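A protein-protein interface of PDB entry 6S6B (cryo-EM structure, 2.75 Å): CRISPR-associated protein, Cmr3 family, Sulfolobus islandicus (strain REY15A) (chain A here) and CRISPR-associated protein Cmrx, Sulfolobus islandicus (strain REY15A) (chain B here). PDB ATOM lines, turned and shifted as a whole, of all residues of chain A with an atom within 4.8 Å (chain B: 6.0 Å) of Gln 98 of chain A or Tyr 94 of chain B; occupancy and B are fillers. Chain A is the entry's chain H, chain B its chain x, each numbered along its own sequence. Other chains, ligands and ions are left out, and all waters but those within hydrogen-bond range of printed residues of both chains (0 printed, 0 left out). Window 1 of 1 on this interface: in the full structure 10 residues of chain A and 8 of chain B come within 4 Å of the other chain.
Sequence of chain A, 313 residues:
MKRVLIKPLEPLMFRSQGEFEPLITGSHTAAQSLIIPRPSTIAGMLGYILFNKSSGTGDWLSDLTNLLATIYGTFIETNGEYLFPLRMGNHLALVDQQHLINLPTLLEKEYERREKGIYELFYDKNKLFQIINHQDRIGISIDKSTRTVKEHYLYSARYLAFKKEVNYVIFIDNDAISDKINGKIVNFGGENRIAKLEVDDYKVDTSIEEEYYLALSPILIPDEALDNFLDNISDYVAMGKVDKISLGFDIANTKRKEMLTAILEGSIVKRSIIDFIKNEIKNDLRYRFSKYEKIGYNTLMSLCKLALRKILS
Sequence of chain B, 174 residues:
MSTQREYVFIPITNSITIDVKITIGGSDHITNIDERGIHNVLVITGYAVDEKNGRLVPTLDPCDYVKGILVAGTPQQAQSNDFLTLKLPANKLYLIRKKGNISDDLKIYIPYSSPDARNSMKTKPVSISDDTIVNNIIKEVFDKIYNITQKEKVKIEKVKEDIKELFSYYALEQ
Printed residues of chain B within 4 Å of Gln 97 of chain A: Tyr 94.
Gln 98 of chain A touches three residues of chain B.
Of the printed residues of chain B, Ile 101 of chain A touches Tyr 94.
Of the printed residues of chain B, Cys 304 of chain A touches Tyr 94 (3.1 Å).
Of the printed residues of chain A, Lys 67 of chain B touches Gln 98 (3.8 Å).
Tyr 94 of chain B touches four residues of chain A.
Printed residues of chain A within 4 Å of Ile 96 of chain B: Gln 98.
The nearest printed residue of chain A that does not touch Tyr 94 of chain B is His 99 of chain A (5.2 Å).
The side-chain amide nitrogen (NE2) of Gln 98 of chain A is in hydrogen-bond range of a ring nitrogen (NE2) of His 99 of chain A (3.3 Å).
The side-chain amide oxygen of Gln 97 of chain A lies close to the backbone carbonyl oxygen of Cys 304 of chain A, at 3.0 Å.
The backbone NH (N) of Val 43 of chain B lies within hydrogen-bond range of the backbone carbonyl oxygen (O) of Tyr 94 of chain B (3.4 Å).
The backbone NH of Val 41 of chain B lies within hydrogen-bond range of the backbone carbonyl oxygen of Ile 96 of chain B (3.3 Å).
Gln 98 of chain A touches Lys 67 of chain B (OE1 to CD, 3.8 Å).
CA of Gln 98 of chain A touches OH of Tyr 94 of chain B (3.3 Å).
Gln 98 of chain A touches Ile 96 of chain B.
Ile 101 of chain A touches Tyr 94 of chain B.
Tyr 94 of chain B touches Cys 304 of chain A.
Of the 7 printed residues of chain A, 4 touch a printed residue of chain B.
Printed residues of chain A that touch a printed residue of chain B: Gln 97, Gln 98, Ile 101 and Cys 304.
Hydrophobic or aromatic side chains of chain A within 4 Å of the printed part of chain B: Ile 101.
Hydrophobic or aromatic side chains of chain B that line the printed part of chain A: Tyr 94 and Ile 96.
Among the printed residues, 6 pairs touch across the chains.
The side-chain amide oxygen (OE1) of Gln 97 of chain A is in hydrogen-bond range of the side-chain hydroxyl (OH) of Tyr 94 of chain B.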
ATOM      1  N   ASP A  96      12.629  22.660  -3.946  1.00  0.00           N
ATOM      2  CA  ASP A  96      12.758  23.918  -4.660  1.00  0.00           C
ATOM      3  C   ASP A  96      13.425  23.703  -6.010  1.00  0.00           C
ATOM      4  O   ASP A  96      14.176  22.745  -6.208  1.00  0.00           O
ATOM      5  CB  ASP A  96      13.559  24.920  -3.833  1.00  0.00           C
ATOM      6  CG  ASP A  96      14.749  24.283  -3.155  1.00  0.00           C
ATOM      7  OD1 ASP A  96      14.934  23.060  -3.315  1.00  0.00           O
ATOM      8  OD2 ASP A  96      15.494  25.001  -2.456  1.00  0.00           O
ATOM      9  N   GLN A  97      13.142  24.616  -6.937  1.00  0.00           N
ATOM     10  CA  GLN A  97      13.562  24.524  -8.331  1.00  0.00           C
ATOM     11  C   GLN A  97      15.041  24.197  -8.501  1.00  0.00           C
ATOM     12  O   GLN A  97      15.411  23.383  -9.352  1.00  0.00           O
ATOM     13  CB  GLN A  97      13.237  25.835  -9.045  1.00  0.00           C
ATOM     14  CG  GLN A  97      14.041  26.079 -10.301  1.00  0.00           C
ATOM     15  CD  GLN A  97      13.710  25.094 -11.397  1.00  0.00           C
ATOM     16  OE1 GLN A  97      14.593  24.435 -11.941  1.00  0.00           O
ATOM     17  NE2 GLN A  97      12.433  24.990 -11.732  1.00  0.00           N
ATOM     18  N   GLN A  98      15.892  24.813  -7.689  1.00  0.00           N
ATOM     19  CA  GLN A  98      17.334  24.716  -7.844  1.00  0.00           C
ATOM     20  C   GLN A  98      17.884  23.330  -7.556  1.00  0.00           C
ATOM     21  O   GLN A  98      19.084  23.109  -7.747  1.00  0.00           O
ATOM     22  CB  GLN A  98      18.025  25.716  -6.922  1.00  0.00           C
ATOM     23  CG  GLN A  98      18.034  25.249  -5.488  1.00  0.00           C
ATOM     24  CD  GLN A  98      19.193  25.806  -4.707  1.00  0.00           C
ATOM     25  OE1 GLN A  98      20.080  26.446  -5.265  1.00  0.00           O
ATOM     26  NE2 GLN A  98      19.206  25.548  -3.407  1.00  0.00           N
ATOM     27  N   HIS A  99      17.062  22.391  -7.094  1.00  0.00           N
ATOM     28  CA  HIS A  99      17.556  21.087  -6.686  1.00  0.00           C
ATOM     29  C   HIS A  99      17.215  19.979  -7.662  1.00  0.00           C
ATOM     30  O   HIS A  99      17.634  18.838  -7.446  1.00  0.00           O
ATOM     31  CB  HIS A  99      17.009  20.716  -5.304  1.00  0.00           C
ATOM     32  CG  HIS A  99      17.697  21.415  -4.178  1.00  0.00           C
ATOM     33  ND1 HIS A  99      17.012  22.085  -3.189  1.00  0.00           N
ATOM     34  CD2 HIS A  99      19.011  21.552  -3.884  1.00  0.00           C
ATOM     35  CE1 HIS A  99      17.873  22.604  -2.334  1.00  0.00           C
ATOM     36  NE2 HIS A  99      19.093  22.297  -2.734  1.00  0.00           N
ATOM     37  N   LEU A 100      16.473  20.275  -8.719  1.00  0.00           N
ATOM     38  CA  LEU A 100      16.167  19.277  -9.730  1.00  0.00           C
ATOM     39  C   LEU A 100      17.229  19.192 -10.812  1.00  0.00           C
ATOM     40  O   LEU A 100      17.239  18.215 -11.564  1.00  0.00           O
ATOM     41  CB  LEU A 100      14.815  19.575 -10.379  1.00  0.00           C
ATOM     42  CG  LEU A 100      13.569  19.551  -9.502  1.00  0.00           C
ATOM     43  CD1 LEU A 100      13.314  20.903  -8.872  1.00  0.00           C
ATOM     44  CD2 LEU A 100      12.386  19.126 -10.333  1.00  0.00           C
ATOM     45  N   ILE A 101      18.118  20.181 -10.896  1.00  0.00           N
ATOM     46  CA  ILE A 101      19.048  20.268 -12.018  1.00  0.00           C
ATOM     47  C   ILE A 101      19.932  19.031 -12.075  1.00  0.00           C
ATOM     48  O   ILE A 101      20.132  18.433 -13.138  1.00  0.00           O
ATOM     49  CB  ILE A 101      19.893  21.546 -11.907  1.00  0.00           C
ATOM     50  CG1 ILE A 101      19.023  22.711 -11.463  1.00  0.00           C
ATOM     51  CG2 ILE A 101      20.541  21.864 -13.234  1.00  0.00           C
ATOM     52  CD1 ILE A 101      19.817  23.835 -10.884  1.00  0.00           C
ATOM     53  N   CYS A 304      15.550  21.518 -16.109  1.00  0.00           N
ATOM     54  CA  CYS A 304      16.203  22.809 -16.309  1.00  0.00           C
ATOM     55  C   CYS A 304      15.457  23.927 -15.606  1.00  0.00           C
ATOM     56  O   CYS A 304      15.961  24.542 -14.660  1.00  0.00           O
ATOM     57  CB  CYS A 304      16.268  23.148 -17.795  1.00  0.00           C
ATOM     58  SG  CYS A 304      17.592  22.531 -18.818  1.00  0.00           S
ATOM     59  N   VAL B  41      19.072  35.669  -7.570  1.00  0.00           N
ATOM     60  CA  VAL B  41      20.369  35.041  -7.361  1.00  0.00           C
ATOM     61  C   VAL B  41      20.607  34.012  -8.456  1.00  0.00           C
ATOM     62  O   VAL B  41      19.700  33.260  -8.826  1.00  0.00           O
ATOM     63  CB  VAL B  41      20.426  34.400  -5.967  1.00  0.00           C
ATOM     64  CG1 VAL B  41      21.728  33.631  -5.774  1.00  0.00           C
ATOM     65  CG2 VAL B  41      20.242  35.453  -4.884  1.00  0.00           C
ATOM     66  N   LEU B  42      21.828  33.973  -8.980  1.00  0.00           N
ATOM     67  CA  LEU B  42      22.167  33.049 -10.054  1.00  0.00           C
ATOM     68  C   LEU B  42      23.131  31.970  -9.568  1.00  0.00           C
ATOM     69  O   LEU B  42      23.934  32.187  -8.657  1.00  0.00           O
ATOM     70  CB  LEU B  42      22.766  33.822 -11.230  1.00  0.00           C
ATOM     71  CG  LEU B  42      23.025  33.141 -12.574  1.00  0.00           C
ATOM     72  CD1 LEU B  42      22.823  34.126 -13.697  1.00  0.00           C
ATOM     73  CD2 LEU B  42      24.434  32.611 -12.631  1.00  0.00           C
ATOM     74  N   VAL B  43      23.052  30.798 -10.198  1.00  0.00           N
ATOM     75  CA  VAL B  43      23.818  29.626  -9.787  1.00  0.00           C
ATOM     76  C   VAL B  43      24.785  29.257 -10.903  1.00  0.00           C
ATOM     77  O   VAL B  43      24.402  29.228 -12.076  1.00  0.00           O
ATOM     78  CB  VAL B  43      22.912  28.423  -9.460  1.00  0.00           C
ATOM     79  CG1 VAL B  43      23.741  27.227  -8.988  1.00  0.00           C
ATOM     80  CG2 VAL B  43      21.878  28.810  -8.420  1.00  0.00           C
ATOM     81  N   TYR B  65      28.776  23.324  -7.692  1.00  0.00           N
ATOM     82  CA  TYR B  65      28.007  24.514  -8.012  1.00  0.00           C
ATOM     83  C   TYR B  65      28.409  25.680  -7.119  1.00  0.00           C
ATOM     84  O   TYR B  65      28.830  25.504  -5.973  1.00  0.00           O
ATOM     85  CB  TYR B  65      26.501  24.233  -7.905  1.00  0.00           C
ATOM     86  CG  TYR B  65      25.985  24.088  -6.492  1.00  0.00           C
ATOM     87  CD1 TYR B  65      26.483  23.110  -5.641  1.00  0.00           C
ATOM     88  CD2 TYR B  65      24.969  24.906  -6.023  1.00  0.00           C
ATOM     89  CE1 TYR B  65      26.003  22.975  -4.355  1.00  0.00           C
ATOM     90  CE2 TYR B  65      24.481  24.772  -4.745  1.00  0.00           C
ATOM     91  CZ  TYR B  65      25.001  23.808  -3.913  1.00  0.00           C
ATOM     92  OH  TYR B  65      24.512  23.682  -2.634  1.00  0.00           O
ATOM     93  N   LYS B  67      27.163  29.898  -6.201  1.00  0.00           N
ATOM     94  CA  LYS B  67      26.054  30.838  -6.277  1.00  0.00           C
ATOM     95  C   LYS B  67      26.493  32.229  -5.835  1.00  0.00           C
ATOM     96  O   LYS B  67      27.184  32.379  -4.823  1.00  0.00           O
ATOM     97  CB  LYS B  67      24.888  30.341  -5.425  1.00  0.00           C
ATOM     98  CG  LYS B  67      24.402  28.970  -5.857  1.00  0.00           C
ATOM     99  CD  LYS B  67      23.252  28.475  -5.019  1.00  0.00           C
ATOM    100  CE  LYS B  67      23.693  28.279  -3.594  1.00  0.00           C
ATOM    101  NZ  LYS B  67      24.943  27.499  -3.499  1.00  0.00           N
ATOM    102  N   ALA B  90      19.148  36.629 -21.544  1.00  0.00           N
ATOM    103  CA  ALA B  90      18.460  36.380 -20.282  1.00  0.00           C
ATOM    104  C   ALA B  90      18.136  34.905 -20.096  1.00  0.00           C
ATOM    105  O   ALA B  90      18.509  34.310 -19.079  1.00  0.00           O
ATOM    106  CB  ALA B  90      17.176  37.201 -20.204  1.00  0.00           C
ATOM    107  N   ASN B  91      17.446  34.301 -21.066  1.00  0.00           N
ATOM    108  CA  ASN B  91      16.952  32.936 -20.931  1.00  0.00           C
ATOM    109  C   ASN B  91      18.049  31.935 -20.603  1.00  0.00           C
ATOM    110  O   ASN B  91      17.735  30.811 -20.200  1.00  0.00           O
ATOM    111  CB  ASN B  91      16.241  32.505 -22.216  1.00  0.00           C
ATOM    112  CG  ASN B  91      14.962  33.284 -22.466  1.00  0.00           C
ATOM    113  OD1 ASN B  91      14.226  33.605 -21.534  1.00  0.00           O
ATOM    114  ND2 ASN B  91      14.683  33.576 -23.732  1.00  0.00           N
ATOM    115  N   LYS B  92      19.314  32.310 -20.754  1.00  0.00           N
ATOM    116  CA  LYS B  92      20.426  31.442 -20.407  1.00  0.00           C
ATOM    117  C   LYS B  92      21.063  31.806 -19.074  1.00  0.00           C
ATOM    118  O   LYS B  92      22.068  31.198 -18.692  1.00  0.00           O
ATOM    119  CB  LYS B  92      21.467  31.470 -21.521  1.00  0.00           C
ATOM    120  CG  LYS B  92      20.915  30.975 -22.837  1.00  0.00           C
ATOM    121  CD  LYS B  92      21.963  30.915 -23.914  1.00  0.00           C
ATOM    122  CE  LYS B  92      21.322  30.538 -25.226  1.00  0.00           C
ATOM    123  NZ  LYS B  92      20.760  29.163 -25.189  1.00  0.00           N
ATOM    124  N   LEU B  93      20.519  32.792 -18.369  1.00  0.00           N
ATOM    125  CA  LEU B  93      20.929  33.078 -17.004  1.00  0.00           C
ATOM    126  C   LEU B  93      20.002  32.332 -16.052  1.00  0.00           C
ATOM    127  O   LEU B  93      18.884  32.785 -15.787  1.00  0.00           O
ATOM    128  CB  LEU B  93      20.879  34.581 -16.723  1.00  0.00           C
ATOM    129  CG  LEU B  93      21.880  35.497 -17.433  1.00  0.00           C
ATOM    130  CD1 LEU B  93      21.544  36.965 -17.183  1.00  0.00           C
ATOM    131  CD2 LEU B  93      23.306  35.194 -17.005  1.00  0.00           C
ATOM    132  N   TYR B  94      20.463  31.192 -15.544  1.00  0.00           N
ATOM    133  CA  TYR B  94      19.649  30.381 -14.639  1.00  0.00           C
ATOM    134  C   TYR B  94      19.632  31.052 -13.274  1.00  0.00           C
ATOM    135  O   TYR B  94      20.619  31.015 -12.536  1.00  0.00           O
ATOM    136  CB  TYR B  94      20.192  28.961 -14.540  1.00  0.00           C
ATOM    137  CG  TYR B  94      19.381  28.099 -13.606  1.00  0.00           C
ATOM    138  CD1 TYR B  94      18.177  27.543 -14.013  1.00  0.00           C
ATOM    139  CD2 TYR B  94      19.802  27.870 -12.305  1.00  0.00           C
ATOM    140  CE1 TYR B  94      17.428  26.763 -13.156  1.00  0.00           C
ATOM    141  CE2 TYR B  94      19.059  27.100 -11.443  1.00  0.00           C
ATOM    142  CZ  TYR B  94      17.875  26.546 -11.873  1.00  0.00           C
ATOM    143  OH  TYR B  94      17.134  25.773 -11.013  1.00  0.00           O
ATOM    144  N   LEU B  95      18.496  31.638 -12.916  1.00  0.00           N
ATOM    145  CA  LEU B  95      18.399  32.482 -11.737  1.00  0.00           C
ATOM    146  C   LEU B  95      17.431  31.886 -10.723  1.00  0.00           C
ATOM    147  O   LEU B  95      16.556  31.083 -11.056  1.00  0.00           O
ATOM    148  CB  LEU B  95      17.941  33.897 -12.112  1.00  0.00           C
ATOM    149  CG  LEU B  95      18.810  34.720 -13.062  1.00  0.00           C
ATOM    150  CD1 LEU B  95      17.939  35.625 -13.911  1.00  0.00           C
ATOM    151  CD2 LEU B  95      19.804  35.543 -12.276  1.00  0.00           C
ATOM    152  N   ILE B  96      17.600  32.312  -9.474  1.00  0.00           N
ATOM    153  CA  ILE B  96      16.715  31.947  -8.374  1.00  0.00           C
ATOM    154  C   ILE B  96      15.872  33.176  -8.057  1.00  0.00           C
ATOM    155  O   ILE B  96      16.220  34.284  -8.471  1.00  0.00           O
ATOM    156  CB  ILE B  96      17.522  31.473  -7.150  1.00  0.00           C
ATOM    157  CG1 ILE B  96      18.685  30.582  -7.590  1.00  0.00           C
ATOM    158  CG2 ILE B  96      16.649  30.717  -6.170  1.00  0.00           C
ATOM    159  CD1 ILE B  96      18.249  29.287  -8.219  1.00  0.00           C
ATOM    160  N   GLU B 165      20.608  30.470   4.119  1.00  0.00           N
ATOM    161  CA  GLU B 165      19.618  29.638   3.455  1.00  0.00           C
ATOM    162  C   GLU B 165      19.838  29.500   1.957  1.00  0.00           C
ATOM    163  O   GLU B 165      19.654  28.403   1.423  1.00  0.00           O
ATOM    164  CB  GLU B 165      18.211  30.208   3.685  1.00  0.00           C
ATOM    165  CG  GLU B 165      17.092  29.415   3.047  1.00  0.00           C
ATOM    166  CD  GLU B 165      15.738  30.050   3.270  1.00  0.00           C
ATOM    167  OE1 GLU B 165      15.683  31.124   3.903  1.00  0.00           O
ATOM    168  OE2 GLU B 165      14.728  29.478   2.810  1.00  0.00           O
ATOM    169  N   LEU B 166      20.241  30.570   1.271  1.00  0.00           N
ATOM    170  CA  LEU B 166      20.354  30.574  -0.182  1.00  0.00           C
ATOM    171  C   LEU B 166      21.718  30.117  -0.670  1.00  0.00           C
ATOM    172  O   LEU B 166      21.809  29.123  -1.393  1.00  0.00           O
ATOM    173  CB  LEU B 166      20.060  31.974  -0.742  1.00  0.00           C
ATOM    174  CG  LEU B 166      18.603  32.341  -1.041  1.00  0.00           C
ATOM    175  CD1 LEU B 166      18.054  31.426  -2.120  1.00  0.00           C
ATOM    176  CD2 LEU B 166      17.723  32.307   0.207  1.00  0.00           C
